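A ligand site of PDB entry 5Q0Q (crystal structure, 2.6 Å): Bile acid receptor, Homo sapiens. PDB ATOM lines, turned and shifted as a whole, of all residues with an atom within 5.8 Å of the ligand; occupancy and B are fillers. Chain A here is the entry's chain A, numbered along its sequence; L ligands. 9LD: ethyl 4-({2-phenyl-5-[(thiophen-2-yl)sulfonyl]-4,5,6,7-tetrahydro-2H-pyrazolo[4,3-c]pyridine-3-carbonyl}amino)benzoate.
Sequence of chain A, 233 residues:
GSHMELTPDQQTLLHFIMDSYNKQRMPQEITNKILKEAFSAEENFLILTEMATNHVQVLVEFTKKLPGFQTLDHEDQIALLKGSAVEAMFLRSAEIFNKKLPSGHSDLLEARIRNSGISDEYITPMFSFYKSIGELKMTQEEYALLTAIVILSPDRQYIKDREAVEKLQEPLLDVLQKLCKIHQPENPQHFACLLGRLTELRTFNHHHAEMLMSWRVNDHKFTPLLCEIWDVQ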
ATOM      1  N   GLN A  24     -15.225  10.128  -2.618  1.00  0.00           N
ATOM      2  CA  GLN A  24     -15.755  11.252  -3.393  1.00  0.00           C
ATOM      3  C   GLN A  24     -16.208  12.418  -2.527  1.00  0.00           C
ATOM      4  O   GLN A  24     -17.077  12.265  -1.648  1.00  0.00           O
ATOM      5  CB  GLN A  24     -16.869  10.784  -4.323  1.00  0.00           C
ATOM      6  CG  GLN A  24     -16.299  10.083  -5.557  1.00  0.00           C
ATOM      7  CD  GLN A  24     -17.292   9.260  -6.319  1.00  0.00           C
ATOM      8  OE1 GLN A  24     -18.497   9.205  -6.007  1.00  0.00           O
ATOM      9  NE2 GLN A  24     -16.789   8.592  -7.354  1.00  0.00           N
ATOM     10  N   ARG A  25     -15.566  13.585  -2.741  1.00  0.00           N
ATOM     11  CA  ARG A  25     -15.818  14.816  -2.003  1.00  0.00           C
ATOM     12  C   ARG A  25     -15.799  16.028  -2.938  1.00  0.00           C
ATOM     13  O   ARG A  25     -15.189  15.981  -4.009  1.00  0.00           O
ATOM     14  CB  ARG A  25     -14.758  15.030  -0.900  1.00  0.00           C
ATOM     15  CG  ARG A  25     -14.811  14.051   0.269  1.00  0.00           C
ATOM     16  CD  ARG A  25     -13.873  14.506   1.370  1.00  0.00           C
ATOM     17  NE  ARG A  25     -13.237  13.393   2.069  1.00  0.00           N
ATOM     18  CZ  ARG A  25     -12.349  13.533   3.054  1.00  0.00           C
ATOM     19  NH1 ARG A  25     -11.992  14.745   3.464  1.00  0.00           N
ATOM     20  NH2 ARG A  25     -11.818  12.461   3.628  1.00  0.00           N
ATOM     21  N   MET A  26     -16.458  17.114  -2.496  1.00  0.00           N
ATOM     22  CA  MET A  26     -16.479  18.381  -3.216  1.00  0.00           C
ATOM     23  C   MET A  26     -15.126  19.075  -2.939  1.00  0.00           C
ATOM     24  O   MET A  26     -14.763  19.203  -1.768  1.00  0.00           O
ATOM     25  CB  MET A  26     -17.652  19.248  -2.742  1.00  0.00           C
ATOM     26  CG  MET A  26     -17.784  20.563  -3.483  1.00  0.00           C
ATOM     27  SD  MET A  26     -18.514  20.392  -5.125  1.00  0.00           S
ATOM     28  CE  MET A  26     -20.239  20.305  -4.676  1.00  0.00           C
ATOM     29  N   PRO A  27     -14.374  19.507  -3.979  1.00  0.00           N
ATOM     30  CA  PRO A  27     -13.073  20.157  -3.734  1.00  0.00           C
ATOM     31  C   PRO A  27     -13.179  21.509  -3.012  1.00  0.00           C
ATOM     32  O   PRO A  27     -14.140  22.253  -3.213  1.00  0.00           O
ATOM     33  CB  PRO A  27     -12.478  20.311  -5.135  1.00  0.00           C
ATOM     34  CG  PRO A  27     -13.284  19.389  -6.018  1.00  0.00           C
ATOM     35  CD  PRO A  27     -14.644  19.404  -5.428  1.00  0.00           C
ATOM     36  N   PHE A  45     -24.033  31.375 -11.787  1.00  0.00           N
ATOM     37  CA  PHE A  45     -24.186  30.380 -12.849  1.00  0.00           C
ATOM     38  C   PHE A  45     -22.857  29.662 -13.118  1.00  0.00           C
ATOM     39  O   PHE A  45     -22.880  28.470 -13.423  1.00  0.00           O
ATOM     40  CB  PHE A  45     -24.675  31.060 -14.133  1.00  0.00           C
ATOM     41  CG  PHE A  45     -25.124  30.124 -15.224  1.00  0.00           C
ATOM     42  CD1 PHE A  45     -26.451  29.707 -15.315  1.00  0.00           C
ATOM     43  CD2 PHE A  45     -24.233  29.671 -16.194  1.00  0.00           C
ATOM     44  CE1 PHE A  45     -26.871  28.852 -16.326  1.00  0.00           C
ATOM     45  CE2 PHE A  45     -24.653  28.816 -17.204  1.00  0.00           C
ATOM     46  CZ  PHE A  45     -25.972  28.428 -17.272  1.00  0.00           C
ATOM     47  N   LEU A  48     -22.052  26.973 -10.499  1.00  0.00           N
ATOM     48  CA  LEU A  48     -22.890  25.800 -10.786  1.00  0.00           C
ATOM     49  C   LEU A  48     -22.317  24.966 -11.926  1.00  0.00           C
ATOM     50  O   LEU A  48     -22.387  23.741 -11.854  1.00  0.00           O
ATOM     51  CB  LEU A  48     -24.363  26.181 -11.050  1.00  0.00           C
ATOM     52  CG  LEU A  48     -25.141  26.818  -9.894  1.00  0.00           C
ATOM     53  CD1 LEU A  48     -26.523  27.209 -10.359  1.00  0.00           C
ATOM     54  CD2 LEU A  48     -25.264  25.872  -8.700  1.00  0.00           C
ATOM     55  N   THR A  49     -21.718  25.618 -12.948  1.00  0.00           N
ATOM     56  CA  THR A  49     -21.062  24.946 -14.070  1.00  0.00           C
ATOM     57  C   THR A  49     -19.828  24.201 -13.565  1.00  0.00           C
ATOM     58  O   THR A  49     -19.684  23.028 -13.894  1.00  0.00           O
ATOM     59  CB  THR A  49     -20.793  25.936 -15.230  1.00  0.00           C
ATOM     60  OG1 THR A  49     -22.039  26.471 -15.670  1.00  0.00           O
ATOM     61  CG2 THR A  49     -20.091  25.283 -16.412  1.00  0.00           C
ATOM     62  N   MET A  51     -19.310  23.159 -10.478  1.00  0.00           N
ATOM     63  CA  MET A  51     -19.851  22.115  -9.610  1.00  0.00           C
ATOM     64  C   MET A  51     -20.381  20.939 -10.426  1.00  0.00           C
ATOM     65  O   MET A  51     -19.930  19.806 -10.215  1.00  0.00           O
ATOM     66  CB  MET A  51     -20.966  22.678  -8.723  1.00  0.00           C
ATOM     67  CG  MET A  51     -20.470  23.480  -7.567  1.00  0.00           C
ATOM     68  SD  MET A  51     -21.839  24.344  -6.779  1.00  0.00           S
ATOM     69  CE  MET A  51     -21.890  23.516  -5.251  1.00  0.00           C
ATOM     70  N   ALA A  52     -21.305  21.201 -11.386  1.00  0.00           N
ATOM     71  CA  ALA A  52     -21.905  20.188 -12.262  1.00  0.00           C
ATOM     72  C   ALA A  52     -20.832  19.436 -13.090  1.00  0.00           C
ATOM     73  O   ALA A  52     -20.943  18.212 -13.221  1.00  0.00           O
ATOM     74  CB  ALA A  52     -22.943  20.813 -13.169  1.00  0.00           C
ATOM     75  N   ASN A  54     -17.631  18.939 -12.157  1.00  0.00           N
ATOM     76  CA  ASN A  54     -16.962  18.107 -11.166  1.00  0.00           C
ATOM     77  C   ASN A  54     -17.757  16.829 -10.886  1.00  0.00           C
ATOM     78  O   ASN A  54     -17.150  15.773 -10.738  1.00  0.00           O
ATOM     79  CB  ASN A  54     -16.667  18.885  -9.886  1.00  0.00           C
ATOM     80  CG  ASN A  54     -15.786  18.121  -8.927  1.00  0.00           C
ATOM     81  OD1 ASN A  54     -14.583  17.959  -9.125  1.00  0.00           O
ATOM     82  ND2 ASN A  54     -16.377  17.592  -7.874  1.00  0.00           N
ATOM     83  N   HIS A  55     -19.106  16.932 -10.858  1.00  0.00           N
ATOM     84  CA  HIS A  55     -19.985  15.790 -10.627  1.00  0.00           C
ATOM     85  C   HIS A  55     -19.847  14.720 -11.727  1.00  0.00           C
ATOM     86  O   HIS A  55     -19.871  13.530 -11.414  1.00  0.00           O
ATOM     87  CB  HIS A  55     -21.467  16.192 -10.420  1.00  0.00           C
ATOM     88  CG  HIS A  55     -22.345  15.009 -10.208  1.00  0.00           C
ATOM     89  ND1 HIS A  55     -23.029  14.403 -11.258  1.00  0.00           N
ATOM     90  CD2 HIS A  55     -22.506  14.249  -9.094  1.00  0.00           C
ATOM     91  CE1 HIS A  55     -23.609  13.337 -10.742  1.00  0.00           C
ATOM     92  NE2 HIS A  55     -23.331  13.212  -9.439  1.00  0.00           N
ATOM     93  N   VAL A  58     -16.997  12.641 -11.002  1.00  0.00           N
ATOM     94  CA  VAL A  58     -17.357  11.921  -9.775  1.00  0.00           C
ATOM     95  C   VAL A  58     -18.250  10.706 -10.125  1.00  0.00           C
ATOM     96  O   VAL A  58     -18.017   9.612  -9.627  1.00  0.00           O
ATOM     97  CB  VAL A  58     -17.997  12.909  -8.754  1.00  0.00           C
ATOM     98  CG1 VAL A  58     -18.858  12.208  -7.718  1.00  0.00           C
ATOM     99  CG2 VAL A  58     -16.930  13.775  -8.081  1.00  0.00           C
ATOM    100  N   MET A  89     -27.040  13.650 -10.024  1.00  0.00           N
ATOM    101  CA  MET A  89     -26.575  14.973  -9.605  1.00  0.00           C
ATOM    102  C   MET A  89     -27.501  15.581  -8.547  1.00  0.00           C
ATOM    103  O   MET A  89     -26.997  16.070  -7.531  1.00  0.00           O
ATOM    104  CB  MET A  89     -26.436  15.924 -10.794  1.00  0.00           C
ATOM    105  CG  MET A  89     -25.788  17.241 -10.421  1.00  0.00           C
ATOM    106  SD  MET A  89     -26.007  18.526 -11.659  1.00  0.00           S
ATOM    107  CE  MET A  89     -27.760  18.783 -11.586  1.00  0.00           C
ATOM    108  N   PHE A  90     -28.822  15.560  -8.786  1.00  0.00           N
ATOM    109  CA  PHE A  90     -29.779  16.120  -7.833  1.00  0.00           C
ATOM    110  C   PHE A  90     -29.853  15.301  -6.547  1.00  0.00           C
ATOM    111  O   PHE A  90     -30.049  15.874  -5.484  1.00  0.00           O
ATOM    112  CB  PHE A  90     -31.172  16.354  -8.456  1.00  0.00           C
ATOM    113  CG  PHE A  90     -31.177  17.551  -9.361  1.00  0.00           C
ATOM    114  CD1 PHE A  90     -30.959  18.836  -8.856  1.00  0.00           C
ATOM    115  CD2 PHE A  90     -31.373  17.408 -10.728  1.00  0.00           C
ATOM    116  CE1 PHE A  90     -30.918  19.940  -9.699  1.00  0.00           C
ATOM    117  CE2 PHE A  90     -31.344  18.517 -11.576  1.00  0.00           C
ATOM    118  CZ  PHE A  90     -31.116  19.777 -11.057  1.00  0.00           C
ATOM    119  N   ARG A  92     -27.225  13.766  -5.272  1.00  0.00           N
ATOM    120  CA  ARG A  92     -25.983  14.183  -4.616  1.00  0.00           C
ATOM    121  C   ARG A  92     -26.129  15.598  -4.041  1.00  0.00           C
ATOM    122  O   ARG A  92     -25.596  15.873  -2.969  1.00  0.00           O
ATOM    123  CB  ARG A  92     -24.810  14.133  -5.595  1.00  0.00           C
ATOM    124  CG  ARG A  92     -23.447  14.001  -4.907  1.00  0.00           C
ATOM    125  CD  ARG A  92     -23.008  12.551  -4.829  1.00  0.00           C
ATOM    126  NE  ARG A  92     -21.968  12.333  -3.822  1.00  0.00           N
ATOM    127  CZ  ARG A  92     -20.934  11.507  -3.965  1.00  0.00           C
ATOM    128  NH1 ARG A  92     -20.056  11.365  -2.985  1.00  0.00           N
ATOM    129  NH2 ARG A  92     -20.784  10.804  -5.088  1.00  0.00           N
ATOM    130  N   SER A  93     -26.848  16.476  -4.761  1.00  0.00           N
ATOM    131  CA  SER A  93     -27.155  17.859  -4.378  1.00  0.00           C
ATOM    132  C   SER A  93     -28.005  17.871  -3.112  1.00  0.00           C
ATOM    133  O   SER A  93     -27.774  18.701  -2.237  1.00  0.00           O
ATOM    134  CB  SER A  93     -27.912  18.569  -5.499  1.00  0.00           C
ATOM    135  OG  SER A  93     -27.100  18.680  -6.659  1.00  0.00           O
ATOM    136  N   ALA A  94     -28.970  16.923  -3.017  1.00  0.00           N
ATOM    137  CA  ALA A  94     -29.866  16.746  -1.868  1.00  0.00           C
ATOM    138  C   ALA A  94     -29.055  16.360  -0.630  1.00  0.00           C
ATOM    139  O   ALA A  94     -29.329  16.875   0.454  1.00  0.00           O
ATOM    140  CB  ALA A  94     -30.904  15.683  -2.160  1.00  0.00           C
ATOM    141  N   GLU A  95     -28.037  15.499  -0.807  1.00  0.00           N
ATOM    142  CA  GLU A  95     -27.140  15.042   0.248  1.00  0.00           C
ATOM    143  C   GLU A  95     -26.287  16.185   0.800  1.00  0.00           C
ATOM    144  O   GLU A  95     -26.174  16.331   2.015  1.00  0.00           O
ATOM    145  CB  GLU A  95     -26.250  13.903  -0.279  1.00  0.00           C
ATOM    146  CG  GLU A  95     -25.411  13.221   0.779  1.00  0.00           C
ATOM    147  CD  GLU A  95     -24.310  12.317   0.274  1.00  0.00           C
ATOM    148  OE1 GLU A  95     -23.697  12.617  -0.777  1.00  0.00           O
ATOM    149  OE2 GLU A  95     -24.025  11.311   0.965  1.00  0.00           O
ATOM    150  N   ILE A  96     -25.705  16.995  -0.096  1.00  0.00           N
ATOM    151  CA  ILE A  96     -24.857  18.141   0.227  1.00  0.00           C
ATOM    152  C   ILE A  96     -25.674  19.270   0.887  1.00  0.00           C
ATOM    153  O   ILE A  96     -25.260  19.789   1.912  1.00  0.00           O
ATOM    154  CB  ILE A  96     -24.047  18.586  -1.035  1.00  0.00           C
ATOM    155  CG1 ILE A  96     -22.847  17.655  -1.245  1.00  0.00           C
ATOM    156  CG2 ILE A  96     -23.591  20.044  -0.960  1.00  0.00           C
ATOM    157  CD1 ILE A  96     -22.312  17.564  -2.635  1.00  0.00           C
ATOM    158  N   PHE A  97     -26.841  19.605   0.308  1.00  0.00           N
ATOM    159  CA  PHE A  97     -27.725  20.659   0.806  1.00  0.00           C
ATOM    160  C   PHE A  97     -28.369  20.354   2.178  1.00  0.00           C
ATOM    161  O   PHE A  97     -28.732  21.296   2.896  1.00  0.00           O
ATOM    162  CB  PHE A  97     -28.804  20.998  -0.239  1.00  0.00           C
ATOM    163  CG  PHE A  97     -29.515  22.302   0.002  1.00  0.00           C
ATOM    164  CD1 PHE A  97     -28.888  23.508  -0.243  1.00  0.00           C
ATOM    165  CD2 PHE A  97     -30.821  22.326   0.482  1.00  0.00           C
ATOM    166  CE1 PHE A  97     -29.540  24.718  -0.012  1.00  0.00           C
ATOM    167  CE2 PHE A  97     -31.474  23.537   0.713  1.00  0.00           C
ATOM    168  CZ  PHE A  97     -30.836  24.718   0.459  1.00  0.00           C
ATOM    169  N   LYS A 100     -23.496  18.031   4.602  1.00  0.00           N
ATOM    170  CA  LYS A 100     -22.155  18.622   4.467  1.00  0.00           C
ATOM    171  C   LYS A 100     -22.143  20.161   4.237  1.00  0.00           C
ATOM    172  O   LYS A 100     -21.937  20.632   3.115  1.00  0.00           O
ATOM    173  CB  LYS A 100     -21.358  17.892   3.362  1.00  0.00           C
ATOM    174  CG  LYS A 100     -21.171  16.401   3.638  1.00  0.00           C
ATOM    175  CD  LYS A 100     -20.835  15.621   2.377  1.00  0.00           C
ATOM    176  CE  LYS A 100     -21.517  14.279   2.333  1.00  0.00           C
ATOM    177  NZ  LYS A 100     -21.049  13.351   3.402  1.00  0.00           N
ATOM    178  N   LEU A 109     -25.488  29.256  -0.761  1.00  0.00           N
ATOM    179  CA  LEU A 109     -25.662  28.465  -1.974  1.00  0.00           C
ATOM    180  C   LEU A 109     -27.090  28.493  -2.467  1.00  0.00           C
ATOM    181  O   LEU A 109     -27.311  28.615  -3.673  1.00  0.00           O
ATOM    182  CB  LEU A 109     -25.144  27.037  -1.793  1.00  0.00           C
ATOM    183  CG  LEU A 109     -25.031  26.141  -3.036  1.00  0.00           C
ATOM    184  CD1 LEU A 109     -24.155  26.755  -4.128  1.00  0.00           C
ATOM    185  CD2 LEU A 109     -24.459  24.833  -2.679  1.00  0.00           C
ATOM    186  N   ILE A 113     -28.210  29.616  -6.112  1.00  0.00           N
ATOM    187  CA  ILE A 113     -29.048  28.779  -6.997  1.00  0.00           C
ATOM    188  C   ILE A 113     -30.287  29.586  -7.433  1.00  0.00           C
ATOM    189  O   ILE A 113     -30.625  29.599  -8.621  1.00  0.00           O
ATOM    190  CB  ILE A 113     -29.423  27.426  -6.325  1.00  0.00           C
ATOM    191  CG1 ILE A 113     -28.179  26.532  -6.084  1.00  0.00           C
ATOM    192  CG2 ILE A 113     -30.502  26.666  -7.138  1.00  0.00           C
ATOM    193  CD1 ILE A 113     -28.298  25.595  -4.890  1.00  0.00           C
ATOM    194  N   ILE A 118     -31.966  30.717 -13.463  1.00  0.00           N
ATOM    195  CA  ILE A 118     -32.838  29.564 -13.689  1.00  0.00           C
ATOM    196  C   ILE A 118     -34.258  29.946 -13.269  1.00  0.00           C
ATOM    197  O   ILE A 118     -34.446  30.505 -12.179  1.00  0.00           O
ATOM    198  CB  ILE A 118     -32.309  28.275 -12.978  1.00  0.00           C
ATOM    199  CG1 ILE A 118     -30.864  27.938 -13.422  1.00  0.00           C
ATOM    200  CG2 ILE A 118     -33.263  27.076 -13.223  1.00  0.00           C
ATOM    201  CD1 ILE A 118     -30.031  27.146 -12.426  1.00  0.00           C
ATOM    202  N   MET A 126     -36.852  21.645  -7.085  1.00  0.00           N
ATOM    203  CA  MET A 126     -35.535  21.292  -6.519  1.00  0.00           C
ATOM    204  C   MET A 126     -35.563  21.290  -4.997  1.00  0.00           C
ATOM    205  O   MET A 126     -35.193  20.291  -4.374  1.00  0.00           O
ATOM    206  CB  MET A 126     -34.428  22.263  -6.978  1.00  0.00           C
ATOM    207  CG  MET A 126     -34.026  22.146  -8.438  1.00  0.00           C
ATOM    208  SD  MET A 126     -32.828  23.445  -8.873  1.00  0.00           S
ATOM    209  CE  MET A 126     -32.894  23.353 -10.649  1.00  0.00           C
ATOM    210  N   TYR A 130     -35.455  18.459  -2.033  1.00  0.00           N
ATOM    211  CA  TYR A 130     -34.422  18.516  -0.981  1.00  0.00           C
ATOM    212  C   TYR A 130     -35.057  18.397   0.411  1.00  0.00           C
ATOM    213  O   TYR A 130     -34.483  17.719   1.273  1.00  0.00           O
ATOM    214  CB  TYR A 130     -33.589  19.803  -1.066  1.00  0.00           C
ATOM    215  CG  TYR A 130     -32.814  20.028  -2.354  1.00  0.00           C
ATOM    216  CD1 TYR A 130     -32.394  18.954  -3.133  1.00  0.00           C
ATOM    217  CD2 TYR A 130     -32.464  21.304  -2.766  1.00  0.00           C
ATOM    218  CE1 TYR A 130     -31.683  19.154  -4.322  1.00  0.00           C
ATOM    219  CE2 TYR A 130     -31.739  21.519  -3.936  1.00  0.00           C
ATOM    220  CZ  TYR A 130     -31.356  20.435  -4.712  1.00  0.00           C
ATOM    221  OH  TYR A 130     -30.651  20.646  -5.874  1.00  0.00           O
ATOM    222  N   HIS A 208     -34.858  19.737 -16.758  1.00  0.00           N
ATOM    223  CA  HIS A 208     -33.490  20.016 -17.162  1.00  0.00           C
ATOM    224  C   HIS A 208     -33.384  20.223 -18.677  1.00  0.00           C
ATOM    225  O   HIS A 208     -32.697  21.154 -19.099  1.00  0.00           O
ATOM    226  CB  HIS A 208     -32.520  18.926 -16.645  1.00  0.00           C
ATOM    227  CG  HIS A 208     -31.072  19.252 -16.842  1.00  0.00           C
ATOM    228  ND1 HIS A 208     -30.400  20.137 -15.998  1.00  0.00           N
ATOM    229  CD2 HIS A 208     -30.212  18.809 -17.786  1.00  0.00           C
ATOM    230  CE1 HIS A 208     -29.160  20.186 -16.447  1.00  0.00           C
ATOM    231  NE2 HIS A 208     -28.997  19.402 -17.515  1.00  0.00           N
ATOM    232  N   MET A 211     -34.841  23.581 -19.494  1.00  0.00           N
ATOM    233  CA  MET A 211     -33.897  24.582 -18.997  1.00  0.00           C
ATOM    234  C   MET A 211     -32.765  24.812 -20.027  1.00  0.00           C
ATOM    235  O   MET A 211     -32.356  25.962 -20.234  1.00  0.00           O
ATOM    236  CB  MET A 211     -33.344  24.129 -17.630  1.00  0.00           C
ATOM    237  CG  MET A 211     -32.378  25.083 -16.986  1.00  0.00           C
ATOM    238  SD  MET A 211     -31.216  24.197 -15.916  1.00  0.00           S
ATOM    239  CE  MET A 211     -30.020  23.591 -17.132  1.00  0.00           C
ATOM    240  N   PHE A 222     -21.073  26.532 -21.623  1.00  0.00           N
ATOM    241  CA  PHE A 222     -20.941  25.559 -20.552  1.00  0.00           C
ATOM    242  C   PHE A 222     -19.498  25.036 -20.402  1.00  0.00           C
ATOM    243  O   PHE A 222     -18.563  25.823 -20.240  1.00  0.00           O
ATOM    244  CB  PHE A 222     -21.960  24.399 -20.718  1.00  0.00           C
ATOM    245  CG  PHE A 222     -23.365  24.724 -20.326  1.00  0.00           C
ATOM    246  CD1 PHE A 222     -24.285  25.164 -21.275  1.00  0.00           C
ATOM    247  CD2 PHE A 222     -23.784  24.621 -19.000  1.00  0.00           C
ATOM    248  CE1 PHE A 222     -25.586  25.487 -20.906  1.00  0.00           C
ATOM    249  CE2 PHE A 222     -25.088  24.946 -18.640  1.00  0.00           C
ATOM    250  CZ  PHE A 222     -25.988  25.378 -19.588  1.00  0.00           C
ATOM    251  N   LEU A 226     -19.763  18.750 -19.802  1.00  0.00           N
ATOM    252  CA  LEU A 226     -21.215  18.900 -19.611  1.00  0.00           C
ATOM    253  C   LEU A 226     -21.966  18.772 -20.917  1.00  0.00           C
ATOM    254  O   LEU A 226     -23.024  18.136 -20.954  1.00  0.00           O
ATOM    255  CB  LEU A 226     -21.581  20.236 -18.937  1.00  0.00           C
ATOM    256  CG  LEU A 226     -21.277  20.389 -17.450  1.00  0.00           C
ATOM    257  CD1 LEU A 226     -21.501  21.826 -17.004  1.00  0.00           C
ATOM    258  CD2 LEU A 226     -22.082  19.403 -16.592  1.00  0.00           C
ATOM    259  N   TRP A 230     -24.798  15.931 -21.771  1.00  0.00           N
ATOM    260  CA  TRP A 230     -26.110  16.503 -22.088  1.00  0.00           C
ATOM    261  C   TRP A 230     -26.238  16.589 -23.627  1.00  0.00           C
ATOM    262  O   TRP A 230     -26.470  15.557 -24.255  1.00  0.00           O
ATOM    263  CB  TRP A 230     -26.311  17.878 -21.410  1.00  0.00           C
ATOM    264  CG  TRP A 230     -26.171  17.895 -19.912  1.00  0.00           C
ATOM    265  CD1 TRP A 230     -26.335  16.852 -19.049  1.00  0.00           C
ATOM    266  CD2 TRP A 230     -25.915  19.058 -19.104  1.00  0.00           C
ATOM    267  NE1 TRP A 230     -26.154  17.278 -17.755  1.00  0.00           N
ATOM    268  CE2 TRP A 230     -25.897  18.628 -17.760  1.00  0.00           C
ATOM    269  CE3 TRP A 230     -25.707  20.417 -19.385  1.00  0.00           C
ATOM    270  CZ2 TRP A 230     -25.684  19.507 -16.691  1.00  0.00           C
ATOM    271  CZ3 TRP A 230     -25.489  21.296 -18.328  1.00  0.00           C
ATOM    272  CH2 TRP A 230     -25.473  20.845 -16.999  1.00  0.00           C
HETATM  273  N3  9LD L   1     -26.737  22.271  -7.440  1.00  0.00           N
HETATM  274  C7  9LD L   1     -24.740  21.107  -8.573  1.00  0.00           C
HETATM  275  C8  9LD L   1     -27.820  22.992  -9.148  1.00  0.00           C
HETATM  276  C10 9LD L   1     -26.431  22.223 -11.150  1.00  0.00           C
HETATM  277  C13 9LD L   1     -20.252  16.581  -6.384  1.00  0.00           C
HETATM  278  C17 9LD L   1     -26.526  22.087  -5.977  1.00  0.00           C
HETATM  279  C20 9LD L   1     -21.384  17.493  -6.690  1.00  0.00           C
HETATM  280  C21 9LD L   1     -25.107  23.454 -14.342  1.00  0.00           C
HETATM  281  C22 9LD L   1     -25.271  25.726 -14.765  1.00  0.00           C
HETATM  282  C24 9LD L   1     -24.458  24.651 -14.752  1.00  0.00           C
HETATM  283  C26 9LD L   1     -22.637  17.366  -6.074  1.00  0.00           C
HETATM  284  C34 9LD L   1     -19.701  14.878  -3.182  1.00  0.00           C
HETATM  285  C33 9LD L   1     -19.316  15.784  -4.286  1.00  0.00           C
HETATM  286  O28 9LD L   1     -20.464  15.869  -5.261  1.00  0.00           O
HETATM  287  O23 9LD L   1     -19.265  16.473  -7.064  1.00  0.00           O
HETATM  288  C29 9LD L   1     -23.671  18.234  -6.364  1.00  0.00           C
HETATM  289  C25 9LD L   1     -23.490  19.253  -7.294  1.00  0.00           C
HETATM  290  N11 9LD L   1     -24.607  20.170  -7.595  1.00  0.00           N
HETATM  291  O19 9LD L   1     -23.882  21.326  -9.423  1.00  0.00           O
HETATM  292  C1  9LD L   1     -26.004  21.868  -8.554  1.00  0.00           C
HETATM  293  C2  9LD L   1     -26.693  22.334  -9.685  1.00  0.00           C
HETATM  294  N6  9LD L   1     -27.629  22.641 -11.920  1.00  0.00           N
HETATM  295  C18 9LD L   1     -28.257  23.882 -11.396  1.00  0.00           C
HETATM  296  C16 9LD L   1     -28.851  23.644 -10.010  1.00  0.00           C
HETATM  297  N5  9LD L   1     -27.876  22.968  -7.839  1.00  0.00           N
HETATM  298  C31 9LD L   1     -25.243  22.010  -5.443  1.00  0.00           C
HETATM  299  C36 9LD L   1     -25.067  21.843  -4.083  1.00  0.00           C
HETATM  300  C37 9LD L   1     -26.153  21.743  -3.235  1.00  0.00           C
HETATM  301  C35 9LD L   1     -27.441  21.821  -3.756  1.00  0.00           C
HETATM  302  C32 9LD L   1     -27.630  21.993  -5.120  1.00  0.00           C
HETATM  303  S4  9LD L   1     -27.550  22.492 -13.525  1.00  0.00           S
HETATM  304  O14 9LD L   1     -26.994  21.200 -13.808  1.00  0.00           O
HETATM  305  O15 9LD L   1     -28.833  22.821 -14.055  1.00  0.00           O
HETATM  306  C9  9LD L   1     -26.432  23.695 -14.066  1.00  0.00           C
HETATM  307  S12 9LD L   1     -26.867  25.341 -14.285  1.00  0.00           S
HETATM  308  C30 9LD L   1     -22.246  19.394  -7.914  1.00  0.00           C
HETATM  309  C27 9LD L   1     -21.209  18.524  -7.615  1.00  0.00           C
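N11 of the ligand sits at hydrogen-bond distance from OG of Ser 93.
An oxygen (O19) of the ligand lies within hydrogen-bond range of the backbone NH (N) of Ala 52 (3.2 Å).
An oxygen (O23) of the ligand lies within hydrogen-bond range of the side-chain amide nitrogen (ND2) of Asn 54, 3.2 Å away.
An oxygen (O14) of the ligand lies close to the side-chain sulfur (SD) of Met 89, 3.6 Å away.
SD of Met 211 sits close to O15 of the ligand (3.3 Å).
Merely in contact with the ligand: Arg 25 (3.8 Å), Met 26 (3.6 Å), Phe 45 (3.8 Å), Leu 48 (3.6 Å), Thr 49 (3.2 Å), Met 51 (3.2 Å), His 55 (3.7 Å), Val 58 (3.7 Å), Arg 92 (3.5 Å), Ile 96 (3.5 Å), Phe 97 (3.9 Å), Leu 109 (3.4 Å), Ile 113 (3.7 Å), Ile 118 (3.9 Å), Tyr 130 (3.4 Å), His 208 (3.6 Å), Phe 222 (3.9 Å) and Trp 230 (3.6 Å).
23 residues have an atom within 4 Å of the ligand: Arg 25, Met 26, Phe 45, Leu 48, Thr 49, Met 51, Ala 52, Asn 54, His 55, Val 58, Met 89, Arg 92, Ser 93, Ile 96, Phe 97, Leu 109, Ile 113, Ile 118, Tyr 130, His 208, Met 211, Phe 222 and Trp 230.
NE of Arg 92 is in salt-bridge range of OE1 of Glu 95 (3.5 Å).
The backbone carbonyl oxygen (O) of Phe 45 lies within hydrogen-bond range of the side-chain hydroxyl (OG1) of Thr 49.
The side-chain amide nitrogen (NE2) of Gln 24 lies within hydrogen-bond range of the backbone carbonyl oxygen (O) of Val 58 (2.8 Å).
The backbone carbonyl oxygen (O) of Met 89 is in hydrogen-bond range of the side-chain hydroxyl (OG) of Ser 93, at 2.8 Å.
OE1 of Gln 24 lies within hydrogen-bond range of NH2 of Arg 92, at 2.9 Å.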
